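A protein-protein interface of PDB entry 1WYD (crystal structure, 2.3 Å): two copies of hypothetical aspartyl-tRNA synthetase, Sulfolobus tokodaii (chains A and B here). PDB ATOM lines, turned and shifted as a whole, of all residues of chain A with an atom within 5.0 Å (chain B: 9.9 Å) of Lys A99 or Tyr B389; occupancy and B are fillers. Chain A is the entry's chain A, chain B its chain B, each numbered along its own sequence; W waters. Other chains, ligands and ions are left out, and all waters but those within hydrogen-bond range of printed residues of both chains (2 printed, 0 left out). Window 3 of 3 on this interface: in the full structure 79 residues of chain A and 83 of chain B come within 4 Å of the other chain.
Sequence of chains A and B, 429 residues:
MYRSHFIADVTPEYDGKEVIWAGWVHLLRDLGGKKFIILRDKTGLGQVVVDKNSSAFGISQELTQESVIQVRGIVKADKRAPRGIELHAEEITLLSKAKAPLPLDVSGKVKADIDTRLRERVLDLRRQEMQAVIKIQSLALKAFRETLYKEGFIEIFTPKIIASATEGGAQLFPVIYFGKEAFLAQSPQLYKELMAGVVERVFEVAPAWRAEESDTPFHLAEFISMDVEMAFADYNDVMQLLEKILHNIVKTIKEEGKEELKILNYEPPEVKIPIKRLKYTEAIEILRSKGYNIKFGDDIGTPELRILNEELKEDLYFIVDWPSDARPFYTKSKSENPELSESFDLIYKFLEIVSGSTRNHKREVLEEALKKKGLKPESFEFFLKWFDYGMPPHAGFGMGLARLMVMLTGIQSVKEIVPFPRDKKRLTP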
ATOM      1  N   GLU A  66      -9.073   3.122  23.545  1.00  0.00           N
ATOM      2  CA  GLU A  66     -10.131   3.755  22.742  1.00  0.00           C
ATOM      3  C   GLU A  66     -10.045   5.297  22.571  1.00  0.00           C
ATOM      4  O   GLU A  66     -10.861   5.910  21.879  1.00  0.00           O
ATOM      5  CB  GLU A  66     -11.542   3.283  23.182  1.00  0.00           C
ATOM      6  CG  GLU A  66     -11.860   1.843  22.788  1.00  0.00           C
ATOM      7  CD  GLU A  66     -11.487   1.498  21.342  1.00  0.00           C
ATOM      8  OE1 GLU A  66     -10.432   0.836  21.165  1.00  0.00           O
ATOM      9  OE2 GLU A  66     -12.219   1.902  20.385  1.00  0.00           O
ATOM     10  N   LYS A  97     -10.187  12.161  24.239  1.00  0.00           N
ATOM     11  CA  LYS A  97      -9.959  11.353  25.431  1.00  0.00           C
ATOM     12  C   LYS A  97     -11.200  10.518  25.793  1.00  0.00           C
ATOM     13  O   LYS A  97     -12.295  11.077  25.971  1.00  0.00           O
ATOM     14  CB  LYS A  97      -9.619  12.273  26.598  1.00  0.00           C
ATOM     15  CG  LYS A  97      -9.144  11.559  27.855  1.00  0.00           C
ATOM     16  CD  LYS A  97      -8.539  12.553  28.855  1.00  0.00           C
ATOM     17  CE  LYS A  97      -7.168  12.092  29.342  1.00  0.00           C
ATOM     18  NZ  LYS A  97      -7.291  10.876  30.208  1.00  0.00           N
ATOM     19  N   ALA A  98     -11.031   9.197  25.909  1.00  0.00           N
ATOM     20  CA  ALA A  98     -12.121   8.298  26.299  1.00  0.00           C
ATOM     21  C   ALA A  98     -12.131   8.022  27.811  1.00  0.00           C
ATOM     22  O   ALA A  98     -11.088   7.952  28.428  1.00  0.00           O
ATOM     23  CB  ALA A  98     -12.024   6.992  25.523  1.00  0.00           C
ATOM     24  N   LYS A  99     -13.309   7.848  28.403  1.00  0.00           N
ATOM     25  CA  LYS A  99     -13.419   7.554  29.832  1.00  0.00           C
ATOM     26  C   LYS A  99     -12.877   6.149  30.167  1.00  0.00           C
ATOM     27  O   LYS A  99     -12.892   5.245  29.306  1.00  0.00           O
ATOM     28  CB  LYS A  99     -14.861   7.742  30.324  1.00  0.00           C
ATOM     29  CG  LYS A  99     -15.392   9.185  30.157  1.00  0.00           C
ATOM     30  CD  LYS A  99     -16.172   9.717  31.377  1.00  0.00           C
ATOM     31  CE  LYS A  99     -15.314  10.710  32.208  1.00  0.00           C
ATOM     32  NZ  LYS A  99     -15.461  10.509  33.682  1.00  0.00           N
ATOM     33  N   ALA A 100     -12.357   6.003  31.392  1.00  0.00           N
ATOM     34  CA  ALA A 100     -11.850   4.725  31.914  1.00  0.00           C
ATOM     35  C   ALA A 100     -12.644   4.256  33.170  1.00  0.00           C
ATOM     36  O   ALA A 100     -13.126   5.077  33.924  1.00  0.00           O
ATOM     37  CB  ALA A 100     -10.366   4.832  32.222  1.00  0.00           C
ATOM     38  N   PRO A 101     -12.841   2.956  33.363  1.00  0.00           N
ATOM     39  CA  PRO A 101     -12.458   1.928  32.391  1.00  0.00           C
ATOM     40  C   PRO A 101     -13.533   1.839  31.304  1.00  0.00           C
ATOM     41  O   PRO A 101     -14.584   2.473  31.417  1.00  0.00           O
ATOM     42  CB  PRO A 101     -12.484   0.646  33.238  1.00  0.00           C
ATOM     43  CG  PRO A 101     -13.713   0.894  34.199  1.00  0.00           C
ATOM     44  CD  PRO A 101     -13.522   2.374  34.550  1.00  0.00           C
ATOM     45  N   LEU A 102     -13.258   1.040  30.278  1.00  0.00           N
ATOM     46  CA  LEU A 102     -14.228   0.717  29.237  1.00  0.00           C
ATOM     47  C   LEU A 102     -15.300  -0.238  29.788  1.00  0.00           C
ATOM     48  O   LEU A 102     -14.977  -1.137  30.566  1.00  0.00           O
ATOM     49  CB  LEU A 102     -13.498   0.055  28.071  1.00  0.00           C
ATOM     50  CG  LEU A 102     -12.554   0.845  27.157  1.00  0.00           C
ATOM     51  CD1 LEU A 102     -12.232  -0.084  26.005  1.00  0.00           C
ATOM     52  CD2 LEU A 102     -13.164   2.156  26.651  1.00  0.00           C
ATOM     53  N   PRO A 103     -16.565  -0.026  29.422  1.00  0.00           N
ATOM     54  CA  PRO A 103     -17.651  -0.946  29.803  1.00  0.00           C
ATOM     55  C   PRO A 103     -17.724  -2.222  28.920  1.00  0.00           C
ATOM     56  O   PRO A 103     -18.495  -3.146  29.197  1.00  0.00           O
ATOM     57  CB  PRO A 103     -18.901  -0.086  29.616  1.00  0.00           C
ATOM     58  CG  PRO A 103     -18.534   0.856  28.509  1.00  0.00           C
ATOM     59  CD  PRO A 103     -17.067   1.149  28.682  1.00  0.00           C
ATOM     60  N   GLU A 120     -23.700  -0.830  24.489  1.00  0.00           N
ATOM     61  CA  GLU A 120     -22.423  -0.214  24.083  1.00  0.00           C
ATOM     62  C   GLU A 120     -22.012  -0.598  22.664  1.00  0.00           C
ATOM     63  O   GLU A 120     -20.866  -0.980  22.407  1.00  0.00           O
ATOM     64  CB  GLU A 120     -21.287  -0.500  25.077  1.00  0.00           C
ATOM     65  CG  GLU A 120     -21.525   0.030  26.483  1.00  0.00           C
ATOM     66  CD  GLU A 120     -21.590   1.547  26.566  1.00  0.00           C
ATOM     67  OE1 GLU A 120     -21.927   2.203  25.575  1.00  0.00           O
ATOM     68  OE2 GLU A 120     -21.334   2.106  27.638  1.00  0.00           O
ATOM     69  N   LEU A 123     -18.563   0.416  20.772  1.00  0.00           N
ATOM     70  CA  LEU A 123     -17.381  -0.362  21.130  1.00  0.00           C
ATOM     71  C   LEU A 123     -17.449  -1.776  20.549  1.00  0.00           C
ATOM     72  O   LEU A 123     -16.454  -2.315  20.035  1.00  0.00           O
ATOM     73  CB  LEU A 123     -17.148  -0.379  22.645  1.00  0.00           C
ATOM     74  CG  LEU A 123     -16.822   0.984  23.257  1.00  0.00           C
ATOM     75  CD1 LEU A 123     -16.940   0.953  24.779  1.00  0.00           C
ATOM     76  CD2 LEU A 123     -15.429   1.485  22.800  1.00  0.00           C
ATOM     77  N   ARG A 126     -16.578  -2.074  16.951  1.00  0.00           N
ATOM     78  CA  ARG A 126     -15.160  -1.754  16.708  1.00  0.00           C
ATOM     79  C   ARG A 126     -14.304  -3.022  16.795  1.00  0.00           C
ATOM     80  O   ARG A 126     -13.152  -3.043  16.373  1.00  0.00           O
ATOM     81  CB  ARG A 126     -14.663  -0.718  17.716  1.00  0.00           C
ATOM     82  CG  ARG A 126     -15.122   0.711  17.470  1.00  0.00           C
ATOM     83  CD  ARG A 126     -14.470   1.724  18.434  1.00  0.00           C
ATOM     84  NE  ARG A 126     -14.916   3.080  18.195  1.00  0.00           N
ATOM     85  CZ  ARG A 126     -14.812   4.090  19.056  1.00  0.00           C
ATOM     86  NH1 ARG A 126     -14.233   3.922  20.249  1.00  0.00           N
ATOM     87  NH2 ARG A 126     -15.298   5.285  18.724  1.00  0.00           N
ATOM     88  N   LEU B 194     -21.896   7.676  14.313  1.00  0.00           N
ATOM     89  CA  LEU B 194     -21.520   6.507  15.079  1.00  0.00           C
ATOM     90  C   LEU B 194     -20.694   5.536  14.255  1.00  0.00           C
ATOM     91  O   LEU B 194     -19.667   5.029  14.736  1.00  0.00           O
ATOM     92  CB  LEU B 194     -22.768   5.764  15.628  1.00  0.00           C
ATOM     93  CG  LEU B 194     -23.592   6.508  16.695  1.00  0.00           C
ATOM     94  CD1 LEU B 194     -24.490   5.543  17.428  1.00  0.00           C
ATOM     95  CD2 LEU B 194     -22.720   7.288  17.677  1.00  0.00           C
ATOM     96  N   GLY B 197     -17.482   6.431  13.582  1.00  0.00           N
ATOM     97  CA  GLY B 197     -16.673   6.330  14.781  1.00  0.00           C
ATOM     98  C   GLY B 197     -16.162   4.914  14.946  1.00  0.00           C
ATOM     99  O   GLY B 197     -15.502   4.607  15.920  1.00  0.00           O
ATOM    100  N   VAL B 198     -16.482   4.051  13.992  1.00  0.00           N
ATOM    101  CA  VAL B 198     -16.047   2.673  13.998  1.00  0.00           C
ATOM    102  C   VAL B 198     -15.256   2.333  12.724  1.00  0.00           C
ATOM    103  O   VAL B 198     -14.135   1.807  12.805  1.00  0.00           O
ATOM    104  CB  VAL B 198     -17.220   1.693  14.204  1.00  0.00           C
ATOM    105  CG1 VAL B 198     -18.393   2.378  14.867  1.00  0.00           C
ATOM    106  CG2 VAL B 198     -17.633   1.075  12.961  1.00  0.00           C
ATOM    107  N   HIS B 361     -17.251  16.591  18.852  1.00  0.00           N
ATOM    108  CA  HIS B 361     -16.796  15.243  19.220  1.00  0.00           C
ATOM    109  C   HIS B 361     -16.471  15.093  20.698  1.00  0.00           C
ATOM    110  O   HIS B 361     -16.117  13.997  21.152  1.00  0.00           O
ATOM    111  CB  HIS B 361     -15.615  14.750  18.349  1.00  0.00           C
ATOM    112  CG  HIS B 361     -14.325  15.477  18.586  1.00  0.00           C
ATOM    113  ND1 HIS B 361     -13.460  15.144  19.608  1.00  0.00           N
ATOM    114  CD2 HIS B 361     -13.737  16.500  17.916  1.00  0.00           C
ATOM    115  CE1 HIS B 361     -12.409  15.947  19.572  1.00  0.00           C
ATOM    116  NE2 HIS B 361     -12.555  16.780  18.558  1.00  0.00           N
ATOM    117  N   LYS B 362     -16.613  16.172  21.452  1.00  0.00           N
ATOM    118  CA  LYS B 362     -16.522  16.096  22.905  1.00  0.00           C
ATOM    119  C   LYS B 362     -17.920  16.239  23.509  1.00  0.00           C
ATOM    120  O   LYS B 362     -18.723  17.058  23.059  1.00  0.00           O
ATOM    121  CB  LYS B 362     -15.587  17.180  23.467  1.00  0.00           C
ATOM    122  CG  LYS B 362     -14.082  17.027  23.149  1.00  0.00           C
ATOM    123  CD  LYS B 362     -13.415  18.406  22.918  1.00  0.00           C
ATOM    124  CE  LYS B 362     -11.901  18.338  22.541  1.00  0.00           C
ATOM    125  NZ  LYS B 362     -11.203  17.083  22.982  1.00  0.00           N
ATOM    126  N   ARG B 363     -18.199  15.424  24.516  1.00  0.00           N
ATOM    127  CA  ARG B 363     -19.459  15.466  25.259  1.00  0.00           C
ATOM    128  C   ARG B 363     -19.775  16.869  25.823  1.00  0.00           C
ATOM    129  O   ARG B 363     -20.907  17.361  25.702  1.00  0.00           O
ATOM    130  CB  ARG B 363     -19.434  14.375  26.352  1.00  0.00           C
ATOM    131  CG  ARG B 363     -20.100  14.724  27.696  1.00  0.00           C
ATOM    132  CD  ARG B 363     -20.432  13.489  28.554  1.00  0.00           C
ATOM    133  NE  ARG B 363     -21.866  13.417  28.795  1.00  0.00           N
ATOM    134  CZ  ARG B 363     -22.618  12.336  28.666  1.00  0.00           C
ATOM    135  NH1 ARG B 363     -22.103  11.172  28.302  1.00  0.00           N
ATOM    136  NH2 ARG B 363     -23.913  12.434  28.908  1.00  0.00           N
ATOM    137  N   GLU B 364     -18.760  17.520  26.393  1.00  0.00           N
ATOM    138  CA  GLU B 364     -18.908  18.858  26.989  1.00  0.00           C
ATOM    139  C   GLU B 364     -19.317  19.940  25.979  1.00  0.00           C
ATOM    140  O   GLU B 364     -20.237  20.712  26.235  1.00  0.00           O
ATOM    141  CB  GLU B 364     -17.624  19.279  27.745  1.00  0.00           C
ATOM    142  N   GLU B 381     -29.355  12.064  26.089  1.00  0.00           N
ATOM    143  CA  GLU B 381     -28.377  11.091  26.578  1.00  0.00           C
ATOM    144  C   GLU B 381     -28.103  10.029  25.514  1.00  0.00           C
ATOM    145  O   GLU B 381     -26.952   9.616  25.347  1.00  0.00           O
ATOM    146  CB  GLU B 381     -28.844  10.440  27.894  1.00  0.00           C
ATOM    147  CG  GLU B 381     -27.767   9.777  28.756  1.00  0.00           C
ATOM    148  CD  GLU B 381     -26.392  10.444  28.695  1.00  0.00           C
ATOM    149  OE1 GLU B 381     -26.295  11.687  28.849  1.00  0.00           O
ATOM    150  OE2 GLU B 381     -25.385   9.723  28.522  1.00  0.00           O
ATOM    151  N   PHE B 383     -27.786  10.402  22.502  1.00  0.00           N
ATOM    152  CA  PHE B 383     -26.827  10.941  21.551  1.00  0.00           C
ATOM    153  C   PHE B 383     -25.479  11.230  22.219  1.00  0.00           C
ATOM    154  O   PHE B 383     -24.423  10.937  21.665  1.00  0.00           O
ATOM    155  CB  PHE B 383     -27.415  12.220  20.922  1.00  0.00           C
ATOM    156  CG  PHE B 383     -26.675  12.742  19.704  1.00  0.00           C
ATOM    157  CD1 PHE B 383     -27.319  12.781  18.451  1.00  0.00           C
ATOM    158  CD2 PHE B 383     -25.392  13.271  19.815  1.00  0.00           C
ATOM    159  CE1 PHE B 383     -26.678  13.289  17.313  1.00  0.00           C
ATOM    160  CE2 PHE B 383     -24.735  13.781  18.693  1.00  0.00           C
ATOM    161  CZ  PHE B 383     -25.383  13.793  17.435  1.00  0.00           C
ATOM    162  N   LEU B 384     -25.522  11.818  23.405  1.00  0.00           N
ATOM    163  CA  LEU B 384     -24.326  12.179  24.159  1.00  0.00           C
ATOM    164  C   LEU B 384     -23.422  11.026  24.583  1.00  0.00           C
ATOM    165  O   LEU B 384     -22.189  11.137  24.483  1.00  0.00           O
ATOM    166  CB  LEU B 384     -24.727  12.972  25.391  1.00  0.00           C
ATOM    167  CG  LEU B 384     -25.421  14.299  25.096  1.00  0.00           C
ATOM    168  CD1 LEU B 384     -26.027  14.811  26.412  1.00  0.00           C
ATOM    169  CD2 LEU B 384     -24.427  15.296  24.507  1.00  0.00           C
ATOM    170  N   LYS B 385     -24.032   9.922  25.015  1.00  0.00           N
ATOM    171  CA  LYS B 385     -23.309   8.810  25.648  1.00  0.00           C
ATOM    172  C   LYS B 385     -22.158   8.255  24.827  1.00  0.00           C
ATOM    173  O   LYS B 385     -21.124   7.881  25.388  1.00  0.00           O
ATOM    174  CB  LYS B 385     -24.256   7.640  25.967  1.00  0.00           C
ATOM    175  CG  LYS B 385     -24.797   6.944  24.727  1.00  0.00           C
ATOM    176  CD  LYS B 385     -25.010   5.460  24.978  1.00  0.00           C
ATOM    177  CE  LYS B 385     -26.477   5.171  25.254  1.00  0.00           C
ATOM    178  NZ  LYS B 385     -26.659   3.700  25.288  1.00  0.00           N
ATOM    179  N   TRP B 386     -22.363   8.162  23.512  1.00  0.00           N
ATOM    180  CA  TRP B 386     -21.405   7.519  22.624  1.00  0.00           C
ATOM    181  C   TRP B 386     -20.072   8.252  22.615  1.00  0.00           C
ATOM    182  O   TRP B 386     -19.040   7.631  22.420  1.00  0.00           O
ATOM    183  CB  TRP B 386     -21.960   7.429  21.210  1.00  0.00           C
ATOM    184  CG  TRP B 386     -23.307   6.835  21.157  1.00  0.00           C
ATOM    185  CD1 TRP B 386     -24.484   7.486  20.905  1.00  0.00           C
ATOM    186  CD2 TRP B 386     -23.637   5.452  21.362  1.00  0.00           C
ATOM    187  NE1 TRP B 386     -25.528   6.591  20.954  1.00  0.00           N
ATOM    188  CE2 TRP B 386     -25.039   5.335  21.223  1.00  0.00           C
ATOM    189  CE3 TRP B 386     -22.888   4.297  21.645  1.00  0.00           C
ATOM    190  CZ2 TRP B 386     -25.705   4.124  21.370  1.00  0.00           C
ATOM    191  CZ3 TRP B 386     -23.556   3.080  21.798  1.00  0.00           C
ATOM    192  CH2 TRP B 386     -24.950   3.006  21.654  1.00  0.00           C
ATOM    193  N   PHE B 387     -20.118   9.555  22.887  1.00  0.00           N
ATOM    194  CA  PHE B 387     -18.931  10.438  22.904  1.00  0.00           C
ATOM    195  C   PHE B 387     -18.063  10.345  24.169  1.00  0.00           C
ATOM    196  O   PHE B 387     -17.041  11.017  24.269  1.00  0.00           O
ATOM    197  CB  PHE B 387     -19.346  11.899  22.643  1.00  0.00           C
ATOM    198  CG  PHE B 387     -19.959  12.104  21.290  1.00  0.00           C
ATOM    199  CD1 PHE B 387     -21.263  11.710  21.038  1.00  0.00           C
ATOM    200  CD2 PHE B 387     -19.212  12.639  20.249  1.00  0.00           C
ATOM    201  CE1 PHE B 387     -21.812  11.843  19.797  1.00  0.00           C
ATOM    202  CE2 PHE B 387     -19.781  12.796  19.001  1.00  0.00           C
ATOM    203  CZ  PHE B 387     -21.083  12.379  18.780  1.00  0.00           C
ATOM    204  N   ASP B 388     -18.454   9.489  25.112  1.00  0.00           N
ATOM    205  CA  ASP B 388     -17.583   9.190  26.247  1.00  0.00           C
ATOM    206  C   ASP B 388     -16.456   8.239  25.876  1.00  0.00           C
ATOM    207  O   ASP B 388     -15.493   8.073  26.641  1.00  0.00           O
ATOM    208  CB  ASP B 388     -18.379   8.569  27.402  1.00  0.00           C
ATOM    209  CG  ASP B 388     -19.257   9.573  28.129  1.00  0.00           C
ATOM    210  OD1 ASP B 388     -20.354   9.148  28.574  1.00  0.00           O
ATOM    211  OD2 ASP B 388     -18.965  10.780  28.314  1.00  0.00           O
ATOM    212  N   TYR B 389     -16.574   7.588  24.726  1.00  0.00           N
ATOM    213  CA  TYR B 389     -15.634   6.522  24.411  1.00  0.00           C
ATOM    214  C   TYR B 389     -14.905   6.687  23.076  1.00  0.00           C
ATOM    215  O   TYR B 389     -14.907   5.781  22.235  1.00  0.00           O
ATOM    216  CB  TYR B 389     -16.308   5.164  24.553  1.00  0.00           C
ATOM    217  CG  TYR B 389     -16.880   4.944  25.940  1.00  0.00           C
ATOM    218  CD1 TYR B 389     -18.249   4.760  26.124  1.00  0.00           C
ATOM    219  CD2 TYR B 389     -16.046   4.929  27.067  1.00  0.00           C
ATOM    220  CE1 TYR B 389     -18.776   4.549  27.389  1.00  0.00           C
ATOM    221  CE2 TYR B 389     -16.555   4.748  28.337  1.00  0.00           C
ATOM    222  CZ  TYR B 389     -17.925   4.550  28.501  1.00  0.00           C
ATOM    223  OH  TYR B 389     -18.462   4.351  29.774  1.00  0.00           O
ATOM    224  N   GLY B 390     -14.264   7.842  22.921  1.00  0.00           N
ATOM    225  CA  GLY B 390     -13.381   8.127  21.798  1.00  0.00           C
ATOM    226  C   GLY B 390     -14.075   8.382  20.470  1.00  0.00           C
ATOM    227  O   GLY B 390     -13.843   7.663  19.497  1.00  0.00           O
ATOM    228  N   MET B 391     -14.933   9.391  20.392  1.00  0.00           N
ATOM    229  CA  MET B 391     -15.449   9.724  19.072  1.00  0.00           C
ATOM    230  C   MET B 391     -14.388  10.595  18.407  1.00  0.00           C
ATOM    231  O   MET B 391     -13.885  11.513  19.044  1.00  0.00           O
ATOM    232  CB  MET B 391     -16.797  10.448  19.154  1.00  0.00           C
ATOM    233  CG  MET B 391     -17.998   9.535  19.366  1.00  0.00           C
ATOM    234  SD  MET B 391     -18.220   8.266  18.098  1.00  0.00           S
ATOM    235  CE  MET B 391     -18.996   9.280  16.833  1.00  0.00           C
ATOM    236  N   PRO B 392     -14.026  10.325  17.155  1.00  0.00           N
ATOM    237  CA  PRO B 392     -12.999  11.123  16.483  1.00  0.00           C
ATOM    238  C   PRO B 392     -13.584  12.415  15.918  1.00  0.00           C
ATOM    239  O   PRO B 392     -14.817  12.552  15.843  1.00  0.00           O
ATOM    240  CB  PRO B 392     -12.571  10.206  15.329  1.00  0.00           C
ATOM    241  CG  PRO B 392     -13.814   9.512  14.941  1.00  0.00           C
ATOM    242  CD  PRO B 392     -14.553   9.268  16.266  1.00  0.00           C
HETATM  243  O   HOH W   1     -11.117  14.920  24.781  1.00  0.00           O
HETATM  244  O   HOH W   2     -22.123   4.609  25.856  1.00  0.00           O
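N of Lys A99 sits at hydrogen-bond distance from O of Asp B388, at 2.8 Å.
The guanidinium group of Arg A126 sits at hydrogen-bond distance from the backbone carbonyl oxygen of Gly B197 (2.8 Å).
NH1 of Arg A126 lies within hydrogen-bond range of O of Tyr B389 (2.8 Å).
O of Gly B390 sits at hydrogen-bond distance from NH2 of Arg A126 (2.9 Å).
The side-chain carboxylate (OE2) of Glu A66 is in salt-bridge range of the guanidinium group (NH1) of Arg A126.
OD1 of Asp B388 is in salt-bridge range of NH1 of Arg B363 (2.7 Å).
Glu A66 touches Gly B390.
O of Asp B388 touches CA of Ala A98 (3.4 Å).
Tyr B389 touches Ala A98 (C to CB, 3.8 Å).
Gly B390 touches Ala A98 (N to CB, 3.5 Å).
Lys A99 touches Tyr B389 (O to CE2, 3.8 Å).
CZ of Tyr B389 touches CD of Pro A103 (3.5 Å).
Glu A120 touches Tyr B389.
Of chain B, only Asp B388 and Tyr B389 come within 4 Å of Lys A99.
Ala A98 touches just these residues of chain B: Asp B388, Tyr B389 and Gly B390.
No residue of chain B comes within 4 Å of Ala A100.
Of the printed residues of chain A, Gly B390 touches Glu A66 (3.4 Å), Ala A98 (3.5 Å) and Arg A126 (2.9 Å).
Of the printed residues of chain A, Asp B388 touches Ala A98 and Lys A99.
Printed residues of chain B within 4 Å of Pro A103: Tyr B389 (3.5 Å).
Printed residues of chain A within 4 Å of Gly B197: Arg A126 (2.8 Å).
The nearest residue of chain A that does not touch Tyr B389 is Leu A102 (4.02 Å).
Of the 18 printed residues of chain B, 4 touch a printed residue of chain A.
Printed residues of chain B that touch a printed residue of chain A: Gly B197, Asp B388, Tyr B389 and Gly B390.
Of the 11 printed residues of chain A, 6 touch a printed residue of chain B.
Printed residues of chain A that touch a printed residue of chain B: Glu A66, Ala A98, Lys A99, Pro A103, Glu A120 and Arg A126.
Hydrophobic or aromatic side chains of chain A that line the printed part of chain B: Ala A98 and Pro A103.
Along chain A the printed residues that touch a printed residue of chain B span positions 66 to 126.
Among the printed residues, 11 pairs touch across the chains.
Among the printed residues, no Asp or Glu carboxylate lies within 4 Å of a Lys or Arg side-chain nitrogen of the other chain.
No position is printed for both chains.
Of the 11 pairs that touch across the chains among the printed residues, none has its exchanged pair printed and touching as well.
Water W2 bridges the side-chain carboxylate (OE1) of Glu A120 (2.4 Å) and the backbone carbonyl oxygen (O) of Lys B385 (3.5 Å).
Water W1 lies within hydrogen-bond range of NZ of Lys B362 (2.8 Å) and N of Lys A97 (3.0 Å).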
